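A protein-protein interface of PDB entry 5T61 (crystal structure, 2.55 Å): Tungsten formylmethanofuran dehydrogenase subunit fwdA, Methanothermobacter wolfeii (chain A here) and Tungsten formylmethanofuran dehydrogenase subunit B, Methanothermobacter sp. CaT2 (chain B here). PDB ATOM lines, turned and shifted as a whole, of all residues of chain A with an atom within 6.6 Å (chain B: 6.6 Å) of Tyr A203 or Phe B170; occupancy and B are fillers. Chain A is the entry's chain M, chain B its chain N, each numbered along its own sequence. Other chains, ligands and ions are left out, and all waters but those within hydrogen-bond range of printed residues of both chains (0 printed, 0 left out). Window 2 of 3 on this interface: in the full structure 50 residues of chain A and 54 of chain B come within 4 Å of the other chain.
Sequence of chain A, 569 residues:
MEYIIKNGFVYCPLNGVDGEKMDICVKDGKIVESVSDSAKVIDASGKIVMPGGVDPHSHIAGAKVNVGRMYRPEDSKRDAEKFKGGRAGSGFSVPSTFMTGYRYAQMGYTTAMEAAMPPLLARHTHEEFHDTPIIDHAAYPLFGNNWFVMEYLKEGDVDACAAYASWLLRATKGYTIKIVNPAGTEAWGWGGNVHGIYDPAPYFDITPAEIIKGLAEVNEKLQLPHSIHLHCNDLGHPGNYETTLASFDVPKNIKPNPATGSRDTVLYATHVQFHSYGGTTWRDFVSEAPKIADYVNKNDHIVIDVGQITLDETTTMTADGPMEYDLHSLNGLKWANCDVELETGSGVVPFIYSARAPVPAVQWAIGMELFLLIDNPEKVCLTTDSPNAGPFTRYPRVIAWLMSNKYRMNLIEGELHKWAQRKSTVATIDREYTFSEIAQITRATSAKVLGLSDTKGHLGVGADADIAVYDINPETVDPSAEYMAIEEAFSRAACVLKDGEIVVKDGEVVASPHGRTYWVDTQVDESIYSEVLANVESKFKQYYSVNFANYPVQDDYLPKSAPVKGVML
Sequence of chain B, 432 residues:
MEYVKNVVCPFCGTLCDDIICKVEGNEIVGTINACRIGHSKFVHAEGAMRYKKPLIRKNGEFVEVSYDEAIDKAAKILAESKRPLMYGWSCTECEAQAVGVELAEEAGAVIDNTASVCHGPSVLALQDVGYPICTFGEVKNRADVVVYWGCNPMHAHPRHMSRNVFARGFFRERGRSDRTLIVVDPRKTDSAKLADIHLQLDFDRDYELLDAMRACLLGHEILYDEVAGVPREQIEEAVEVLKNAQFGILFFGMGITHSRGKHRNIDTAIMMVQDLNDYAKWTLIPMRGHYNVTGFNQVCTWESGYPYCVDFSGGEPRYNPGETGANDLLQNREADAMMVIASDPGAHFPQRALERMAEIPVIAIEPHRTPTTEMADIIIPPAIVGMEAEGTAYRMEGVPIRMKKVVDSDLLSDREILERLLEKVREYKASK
The backbone carbonyl oxygen (O) of Gln A542 lies within hydrogen-bond range of the side-chain amino group (NZ) of Lys B140, at 3.1 Å. The side-chain carboxylate (OE1) of Glu A186 is in salt-bridge range of the guanidinium group (NH1) of Arg B142, 2.9 Å away. The side-chain amide oxygen (OD1) of Asn B141 sits close to the backbone carbonyl oxygen (O) of Tyr A543. NE1 of Trp A190 sits close to NH2 of Arg B142, at 2.9 Å.
The side-chain amide nitrogen of Asn B141 sits close to the backbone NH of Phe B170, at 2.9 Å. The indole nitrogen (NE1) of Trp A147 is in hydrogen-bond range of the side-chain carboxylate (OE1) of Glu A186 (3.0 Å). The backbone NH of Phe B171 sits at hydrogen-bond distance from the backbone carbonyl oxygen of Asn B141, at 3.0 Å. The backbone carbonyl oxygen of Arg B142 is in hydrogen-bond range of the guanidinium group of Arg B172.
CG of Phe B170 touches CZ3 of Trp A147 (3.7 Å). CH2 of Trp A147 touches CE2 of Phe B171, at 3.8 Å. Trp A190 touches Phe B171 (CZ2 to CD2, 3.5 Å). Trp A190 touches Arg B172. Phe B170 touches Tyr A203 (CZ to OH, 3.5 Å). Tyr A203 touches Phe B171. CE of Lys B140 touches O of Tyr A543, 3.5 Å away. Tyr A543 touches Phe B170.
Of the printed residues of chain B, Trp A147 touches Phe B170 and Phe B171. Lys A154 touches none of the printed residues of chain B. Of the printed residues of chain B, Glu A186 touches Arg B142 (2.9 Å). Pro A202 touches none of the printed residues of chain B. Tyr A203 touches just these residues of chain B: Phe B170 and Phe B171. Of the printed residues of chain A, Phe B171 touches Trp A147, Trp A190 and Tyr A203. The nearest residue of chain A that does not touch Phe B170 is Lys A539 (4.3 Å). The nearest printed residue of chain B that does not touch Tyr A543 is Gly B169 (4.1 Å).
Printed residues of chain B that touch a printed residue of chain A: Lys B140, Asn B141, Arg B142, Phe B170, Phe B171 and Arg B172. Along chain B the printed residues that touch a printed residue of chain A span positions 140 to 172. Of the 14 printed residues of chain A, 6 touch a printed residue of chain B. Hydrophobic or aromatic side chains of chain A that line the printed part of chain B: Trp A147, Trp A190, Tyr A203 and Tyr A543. Among the printed residues, 12 pairs touch across the chains.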
ATOM      1  N   TRP A 147      -7.524  13.381  -4.393  1.00  0.00           N
ATOM      2  CA  TRP A 147      -6.455  14.374  -4.451  1.00  0.00           C
ATOM      3  C   TRP A 147      -5.691  14.458  -3.133  1.00  0.00           C
ATOM      4  O   TRP A 147      -4.455  14.528  -3.130  1.00  0.00           O
ATOM      5  CB  TRP A 147      -7.025  15.742  -4.826  1.00  0.00           C
ATOM      6  CG  TRP A 147      -7.323  15.893  -6.286  1.00  0.00           C
ATOM      7  CD1 TRP A 147      -7.563  14.893  -7.182  1.00  0.00           C
ATOM      8  CD2 TRP A 147      -7.391  17.120  -7.024  1.00  0.00           C
ATOM      9  NE1 TRP A 147      -7.787  15.423  -8.432  1.00  0.00           N
ATOM     10  CE2 TRP A 147      -7.686  16.788  -8.361  1.00  0.00           C
ATOM     11  CE3 TRP A 147      -7.236  18.467  -6.682  1.00  0.00           C
ATOM     12  CZ2 TRP A 147      -7.831  17.752  -9.357  1.00  0.00           C
ATOM     13  CZ3 TRP A 147      -7.382  19.425  -7.672  1.00  0.00           C
ATOM     14  CH2 TRP A 147      -7.674  19.063  -8.994  1.00  0.00           C
ATOM     15  N   GLU A 151      -1.681  13.528  -2.607  1.00  0.00           N
ATOM     16  CA  GLU A 151      -0.731  14.534  -2.145  1.00  0.00           C
ATOM     17  C   GLU A 151      -0.077  14.122  -0.831  1.00  0.00           C
ATOM     18  O   GLU A 151       1.129  14.326  -0.644  1.00  0.00           O
ATOM     19  CB  GLU A 151      -1.420  15.890  -2.006  1.00  0.00           C
ATOM     20  CG  GLU A 151      -1.675  16.602  -3.331  1.00  0.00           C
ATOM     21  CD  GLU A 151      -0.404  17.127  -3.990  1.00  0.00           C
ATOM     22  OE1 GLU A 151       0.467  16.316  -4.375  1.00  0.00           O
ATOM     23  OE2 GLU A 151      -0.277  18.361  -4.133  1.00  0.00           O
ATOM     24  N   LYS A 154       2.404  10.991  -1.432  1.00  0.00           N
ATOM     25  CA  LYS A 154       3.621  11.325  -2.166  1.00  0.00           C
ATOM     26  C   LYS A 154       4.675  11.911  -1.235  1.00  0.00           C
ATOM     27  O   LYS A 154       5.867  11.612  -1.374  1.00  0.00           O
ATOM     28  CB  LYS A 154       3.310  12.291  -3.310  1.00  0.00           C
ATOM     29  CG  LYS A 154       4.549  12.795  -4.045  1.00  0.00           C
ATOM     30  CD  LYS A 154       4.365  14.233  -4.487  1.00  0.00           C
ATOM     31  CE  LYS A 154       4.224  15.143  -3.277  1.00  0.00           C
ATOM     32  NZ  LYS A 154       3.560  16.431  -3.617  1.00  0.00           N
ATOM     33  N   GLU A 186      -7.774   9.475 -12.325  1.00  0.00           N
ATOM     34  CA  GLU A 186      -7.300  10.854 -12.327  1.00  0.00           C
ATOM     35  C   GLU A 186      -6.684  11.217 -13.671  1.00  0.00           C
ATOM     36  O   GLU A 186      -6.877  12.332 -14.172  1.00  0.00           O
ATOM     37  CB  GLU A 186      -6.298  11.068 -11.190  1.00  0.00           C
ATOM     38  CG  GLU A 186      -5.515  12.358 -11.316  1.00  0.00           C
ATOM     39  CD  GLU A 186      -6.404  13.588 -11.266  1.00  0.00           C
ATOM     40  OE1 GLU A 186      -7.507  13.516 -10.678  1.00  0.00           O
ATOM     41  OE2 GLU A 186      -6.003  14.623 -11.839  1.00  0.00           O
ATOM     42  N   TRP A 190      -8.007  14.031 -17.695  1.00  0.00           N
ATOM     43  CA  TRP A 190      -7.503  14.649 -18.915  1.00  0.00           C
ATOM     44  C   TRP A 190      -7.666  13.753 -20.139  1.00  0.00           C
ATOM     45  O   TRP A 190      -7.115  14.067 -21.198  1.00  0.00           O
ATOM     46  CB  TRP A 190      -6.030  15.038 -18.770  1.00  0.00           C
ATOM     47  CG  TRP A 190      -5.707  15.869 -17.577  1.00  0.00           C
ATOM     48  CD1 TRP A 190      -5.062  15.462 -16.448  1.00  0.00           C
ATOM     49  CD2 TRP A 190      -6.013  17.257 -17.388  1.00  0.00           C
ATOM     50  NE1 TRP A 190      -4.935  16.512 -15.571  1.00  0.00           N
ATOM     51  CE2 TRP A 190      -5.515  17.624 -16.122  1.00  0.00           C
ATOM     52  CE3 TRP A 190      -6.657  18.224 -18.165  1.00  0.00           C
ATOM     53  CZ2 TRP A 190      -5.644  18.915 -15.614  1.00  0.00           C
ATOM     54  CZ3 TRP A 190      -6.781  19.508 -17.660  1.00  0.00           C
ATOM     55  CH2 TRP A 190      -6.277  19.840 -16.396  1.00  0.00           C
ATOM     56  N   ALA A 201       0.196   9.237 -12.408  1.00  0.00           N
ATOM     57  CA  ALA A 201      -0.813  10.142 -12.929  1.00  0.00           C
ATOM     58  C   ALA A 201      -0.183  11.482 -13.287  1.00  0.00           C
ATOM     59  O   ALA A 201       0.877  11.839 -12.768  1.00  0.00           O
ATOM     60  CB  ALA A 201      -1.924  10.335 -11.900  1.00  0.00           C
ATOM     61  N   PRO A 202      -0.806  12.238 -14.194  1.00  0.00           N
ATOM     62  CA  PRO A 202      -0.310  13.588 -14.486  1.00  0.00           C
ATOM     63  C   PRO A 202      -0.304  14.463 -13.241  1.00  0.00           C
ATOM     64  O   PRO A 202      -1.160  14.341 -12.362  1.00  0.00           O
ATOM     65  CB  PRO A 202      -1.295  14.109 -15.538  1.00  0.00           C
ATOM     66  CG  PRO A 202      -1.852  12.880 -16.172  1.00  0.00           C
ATOM     67  CD  PRO A 202      -1.929  11.863 -15.073  1.00  0.00           C
ATOM     68  N   TYR A 203       0.700  15.341 -13.174  1.00  0.00           N
ATOM     69  CA  TYR A 203       0.918  16.297 -12.090  1.00  0.00           C
ATOM     70  C   TYR A 203       1.250  15.658 -10.747  1.00  0.00           C
ATOM     71  O   TYR A 203       2.255  16.013 -10.123  1.00  0.00           O
ATOM     72  CB  TYR A 203      -0.290  17.217 -11.891  1.00  0.00           C
ATOM     73  CG  TYR A 203      -0.104  18.079 -10.666  1.00  0.00           C
ATOM     74  CD1 TYR A 203       0.704  19.204 -10.710  1.00  0.00           C
ATOM     75  CD2 TYR A 203      -0.697  17.743  -9.451  1.00  0.00           C
ATOM     76  CE1 TYR A 203       0.904  19.982  -9.589  1.00  0.00           C
ATOM     77  CE2 TYR A 203      -0.502  18.517  -8.322  1.00  0.00           C
ATOM     78  CZ  TYR A 203       0.300  19.638  -8.400  1.00  0.00           C
ATOM     79  OH  TYR A 203       0.504  20.423  -7.289  1.00  0.00           O
ATOM     80  N   PHE A 204       0.402  14.745 -10.273  1.00  0.00           N
ATOM     81  CA  PHE A 204       0.520  14.295  -8.890  1.00  0.00           C
ATOM     82  C   PHE A 204       1.731  13.395  -8.679  1.00  0.00           C
ATOM     83  O   PHE A 204       2.267  13.339  -7.567  1.00  0.00           O
ATOM     84  CB  PHE A 204      -0.776  13.601  -8.468  1.00  0.00           C
ATOM     85  CG  PHE A 204      -1.944  14.544  -8.328  1.00  0.00           C
ATOM     86  CD1 PHE A 204      -2.101  15.307  -7.181  1.00  0.00           C
ATOM     87  CD2 PHE A 204      -2.864  14.689  -9.353  1.00  0.00           C
ATOM     88  CE1 PHE A 204      -3.167  16.182  -7.049  1.00  0.00           C
ATOM     89  CE2 PHE A 204      -3.931  15.565  -9.230  1.00  0.00           C
ATOM     90  CZ  PHE A 204      -4.083  16.311  -8.076  1.00  0.00           C
ATOM     91  N   ASP A 205       2.176  12.697  -9.725  1.00  0.00           N
ATOM     92  CA  ASP A 205       3.507  12.080  -9.763  1.00  0.00           C
ATOM     93  C   ASP A 205       3.669  11.001  -8.692  1.00  0.00           C
ATOM     94  O   ASP A 205       4.727  10.868  -8.075  1.00  0.00           O
ATOM     95  CB  ASP A 205       4.613  13.132  -9.648  1.00  0.00           C
ATOM     96  CG  ASP A 205       5.971  12.594 -10.074  1.00  0.00           C
ATOM     97  OD1 ASP A 205       6.021  11.767 -11.013  1.00  0.00           O
ATOM     98  OD2 ASP A 205       6.986  12.988  -9.461  1.00  0.00           O
ATOM     99  N   ILE A 206       2.603  10.253  -8.433  1.00  0.00           N
ATOM    100  CA  ILE A 206       2.649   9.119  -7.522  1.00  0.00           C
ATOM    101  C   ILE A 206       2.161   7.891  -8.283  1.00  0.00           C
ATOM    102  O   ILE A 206       1.254   7.989  -9.117  1.00  0.00           O
ATOM    103  CB  ILE A 206       1.810   9.378  -6.252  1.00  0.00           C
ATOM    104  CG1 ILE A 206       1.892   8.196  -5.286  1.00  0.00           C
ATOM    105  CG2 ILE A 206       0.363   9.692  -6.613  1.00  0.00           C
ATOM    106  CD1 ILE A 206       1.262   8.472  -3.936  1.00  0.00           C
ATOM    107  N   LYS A 539      -8.588  23.688   1.039  1.00  0.00           N
ATOM    108  CA  LYS A 539      -8.778  23.299  -0.349  1.00  0.00           C
ATOM    109  C   LYS A 539     -10.247  23.373  -0.752  1.00  0.00           C
ATOM    110  O   LYS A 539     -10.555  23.639  -1.921  1.00  0.00           O
ATOM    111  CB  LYS A 539      -8.202  21.906  -0.580  1.00  0.00           C
ATOM    112  CG  LYS A 539      -6.785  21.765  -0.069  1.00  0.00           C
ATOM    113  CD  LYS A 539      -5.803  21.457  -1.193  1.00  0.00           C
ATOM    114  CE  LYS A 539      -6.077  20.129  -1.870  1.00  0.00           C
ATOM    115  NZ  LYS A 539      -5.393  20.005  -3.190  1.00  0.00           N
ATOM    116  N   GLN A 542     -10.774  26.964  -1.826  1.00  0.00           N
ATOM    117  CA  GLN A 542     -10.149  27.258  -3.111  1.00  0.00           C
ATOM    118  C   GLN A 542     -10.758  26.446  -4.249  1.00  0.00           C
ATOM    119  O   GLN A 542     -11.176  27.006  -5.270  1.00  0.00           O
ATOM    120  CB  GLN A 542      -8.640  26.995  -3.025  1.00  0.00           C
ATOM    121  CG  GLN A 542      -7.883  27.796  -1.983  1.00  0.00           C
ATOM    122  CD  GLN A 542      -6.435  27.364  -1.876  1.00  0.00           C
ATOM    123  OE1 GLN A 542      -6.118  26.389  -1.193  1.00  0.00           O
ATOM    124  NE2 GLN A 542      -5.560  28.031  -2.622  1.00  0.00           N
ATOM    125  N   TYR A 543     -10.837  25.126  -4.087  1.00  0.00           N
ATOM    126  CA  TYR A 543     -10.914  24.226  -5.225  1.00  0.00           C
ATOM    127  C   TYR A 543     -12.200  23.418  -5.320  1.00  0.00           C
ATOM    128  O   TYR A 543     -12.543  22.977  -6.423  1.00  0.00           O
ATOM    129  CB  TYR A 543      -9.714  23.262  -5.199  1.00  0.00           C
ATOM    130  CG  TYR A 543      -8.365  23.967  -5.232  1.00  0.00           C
ATOM    131  CD1 TYR A 543      -8.090  24.947  -6.182  1.00  0.00           C
ATOM    132  CD2 TYR A 543      -7.375  23.666  -4.302  1.00  0.00           C
ATOM    133  CE1 TYR A 543      -6.861  25.594  -6.215  1.00  0.00           C
ATOM    134  CE2 TYR A 543      -6.144  24.309  -4.325  1.00  0.00           C
ATOM    135  CZ  TYR A 543      -5.892  25.271  -5.282  1.00  0.00           C
ATOM    136  OH  TYR A 543      -4.671  25.910  -5.307  1.00  0.00           O
ATOM    137  N   LYS B 140     -14.190  24.142 -13.016  1.00  0.00           N
ATOM    138  CA  LYS B 140     -13.427  25.247 -12.439  1.00  0.00           C
ATOM    139  C   LYS B 140     -11.929  24.973 -12.444  1.00  0.00           C
ATOM    140  O   LYS B 140     -11.132  25.874 -12.736  1.00  0.00           O
ATOM    141  CB  LYS B 140     -13.938  25.554 -11.027  1.00  0.00           C
ATOM    142  CG  LYS B 140     -13.069  26.519 -10.241  1.00  0.00           C
ATOM    143  CD  LYS B 140     -13.776  26.953  -8.963  1.00  0.00           C
ATOM    144  CE  LYS B 140     -13.540  26.049  -7.774  1.00  0.00           C
ATOM    145  NZ  LYS B 140     -13.988  26.756  -6.539  1.00  0.00           N
ATOM    146  N   ASN B 141     -11.516  23.750 -12.118  1.00  0.00           N
ATOM    147  CA  ASN B 141     -10.101  23.494 -11.942  1.00  0.00           C
ATOM    148  C   ASN B 141      -9.421  22.998 -13.218  1.00  0.00           C
ATOM    149  O   ASN B 141      -8.184  23.051 -13.304  1.00  0.00           O
ATOM    150  CB  ASN B 141      -9.904  22.490 -10.790  1.00  0.00           C
ATOM    151  CG  ASN B 141     -10.479  23.010  -9.470  1.00  0.00           C
ATOM    152  OD1 ASN B 141     -11.351  22.377  -8.877  1.00  0.00           O
ATOM    153  ND2 ASN B 141     -10.024  24.169  -9.032  1.00  0.00           N
ATOM    154  N   ARG B 142     -10.183  22.528 -14.216  1.00  0.00           N
ATOM    155  CA  ARG B 142      -9.558  21.939 -15.395  1.00  0.00           C
ATOM    156  C   ARG B 142      -9.950  22.597 -16.712  1.00  0.00           C
ATOM    157  O   ARG B 142      -9.183  22.531 -17.682  1.00  0.00           O
ATOM    158  CB  ARG B 142      -9.920  20.457 -15.512  1.00  0.00           C
ATOM    159  CG  ARG B 142      -9.719  19.621 -14.276  1.00  0.00           C
ATOM    160  CD  ARG B 142      -8.980  18.346 -14.618  1.00  0.00           C
ATOM    161  NE  ARG B 142      -9.243  17.310 -13.629  1.00  0.00           N
ATOM    162  CZ  ARG B 142      -8.542  16.189 -13.521  1.00  0.00           C
ATOM    163  NH1 ARG B 142      -8.860  15.293 -12.598  1.00  0.00           N
ATOM    164  NH2 ARG B 142      -7.510  15.975 -14.322  1.00  0.00           N
ATOM    165  N   ARG B 168     -10.735  31.048 -10.250  1.00  0.00           N
ATOM    166  CA  ARG B 168      -9.372  30.562 -10.405  1.00  0.00           C
ATOM    167  C   ARG B 168      -9.289  29.143  -9.855  1.00  0.00           C
ATOM    168  O   ARG B 168      -9.530  28.918  -8.664  1.00  0.00           O
ATOM    169  CB  ARG B 168      -8.387  31.479  -9.682  1.00  0.00           C
ATOM    170  CG  ARG B 168      -8.334  32.896 -10.228  1.00  0.00           C
ATOM    171  CD  ARG B 168      -7.753  33.844  -9.191  1.00  0.00           C
ATOM    172  NE  ARG B 168      -7.895  35.246  -9.572  1.00  0.00           N
ATOM    173  CZ  ARG B 168      -9.008  35.958  -9.421  1.00  0.00           C
ATOM    174  NH1 ARG B 168     -10.098  35.401  -8.909  1.00  0.00           N
ATOM    175  NH2 ARG B 168      -9.033  37.232  -9.792  1.00  0.00           N
ATOM    176  N   GLY B 169      -8.962  28.190 -10.727  1.00  0.00           N
ATOM    177  CA  GLY B 169      -8.899  26.794 -10.369  1.00  0.00           C
ATOM    178  C   GLY B 169      -7.474  26.276 -10.238  1.00  0.00           C
ATOM    179  O   GLY B 169      -6.493  26.974 -10.479  1.00  0.00           O
ATOM    180  N   PHE B 170      -7.393  25.006  -9.830  1.00  0.00           N
ATOM    181  CA  PHE B 170      -6.107  24.370  -9.543  1.00  0.00           C
ATOM    182  C   PHE B 170      -5.185  24.405 -10.757  1.00  0.00           C
ATOM    183  O   PHE B 170      -4.041  24.868 -10.671  1.00  0.00           O
ATOM    184  CB  PHE B 170      -6.342  22.938  -9.057  1.00  0.00           C
ATOM    185  CG  PHE B 170      -5.126  22.287  -8.458  1.00  0.00           C
ATOM    186  CD1 PHE B 170      -4.779  22.523  -7.138  1.00  0.00           C
ATOM    187  CD2 PHE B 170      -4.360  21.401  -9.198  1.00  0.00           C
ATOM    188  CE1 PHE B 170      -3.666  21.920  -6.579  1.00  0.00           C
ATOM    189  CE2 PHE B 170      -3.250  20.789  -8.642  1.00  0.00           C
ATOM    190  CZ  PHE B 170      -2.903  21.050  -7.331  1.00  0.00           C
ATOM    191  N   PHE B 171      -5.664  23.923 -11.900  1.00  0.00           N
ATOM    192  CA  PHE B 171      -4.896  23.969 -13.136  1.00  0.00           C
ATOM    193  C   PHE B 171      -5.232  25.203 -13.958  1.00  0.00           C
ATOM    194  O   PHE B 171      -4.674  25.382 -15.047  1.00  0.00           O
ATOM    195  CB  PHE B 171      -5.141  22.705 -13.971  1.00  0.00           C
ATOM    196  CG  PHE B 171      -4.771  21.426 -13.271  1.00  0.00           C
ATOM    197  CD1 PHE B 171      -3.466  20.962 -13.282  1.00  0.00           C
ATOM    198  CD2 PHE B 171      -5.732  20.689 -12.598  1.00  0.00           C
ATOM    199  CE1 PHE B 171      -3.129  19.779 -12.644  1.00  0.00           C
ATOM    200  CE2 PHE B 171      -5.401  19.506 -11.955  1.00  0.00           C
ATOM    201  CZ  PHE B 171      -4.098  19.052 -11.979  1.00  0.00           C
ATOM    202  N   ARG B 172      -6.126  26.059 -13.456  1.00  0.00           N
ATOM    203  CA  ARG B 172      -6.525  27.277 -14.151  1.00  0.00           C
ATOM    204  C   ARG B 172      -6.411  28.490 -13.214  1.00  0.00           C
ATOM    205  O   ARG B 172      -7.384  29.219 -13.021  1.00  0.00           O
ATOM    206  CB  ARG B 172      -7.953  27.176 -14.705  1.00  0.00           C
ATOM    207  CG  ARG B 172      -8.211  25.978 -15.603  1.00  0.00           C
ATOM    208  CD  ARG B 172      -7.394  25.952 -16.874  1.00  0.00           C
ATOM    209  NE  ARG B 172      -7.501  24.620 -17.456  1.00  0.00           N
ATOM    210  CZ  ARG B 172      -6.546  24.035 -18.166  1.00  0.00           C
ATOM    211  NH1 ARG B 172      -5.409  24.675 -18.396  1.00  0.00           N
ATOM    212  NH2 ARG B 172      -6.733  22.812 -18.644  1.00  0.00           N
ATOM    213  N   GLU B 173      -5.205  28.752 -12.671  1.00  0.00           N
ATOM    214  CA  GLU B 173      -5.070  29.874 -11.738  1.00  0.00           C
ATOM    215  C   GLU B 173      -5.389  31.218 -12.299  1.00  0.00           C
ATOM    216  O   GLU B 173      -5.592  32.137 -11.506  1.00  0.00           O
ATOM    217  CB  GLU B 173      -3.680  30.139 -11.167  1.00  0.00           C
ATOM    218  CG  GLU B 173      -3.634  30.039  -9.645  1.00  0.00           C
ATOM    219  CD  GLU B 173      -2.236  30.279  -9.129  1.00  0.00           C
ATOM    220  OE1 GLU B 173      -1.323  29.767  -9.807  1.00  0.00           O
ATOM    221  OE2 GLU B 173      -2.045  31.059  -8.157  1.00  0.00           O
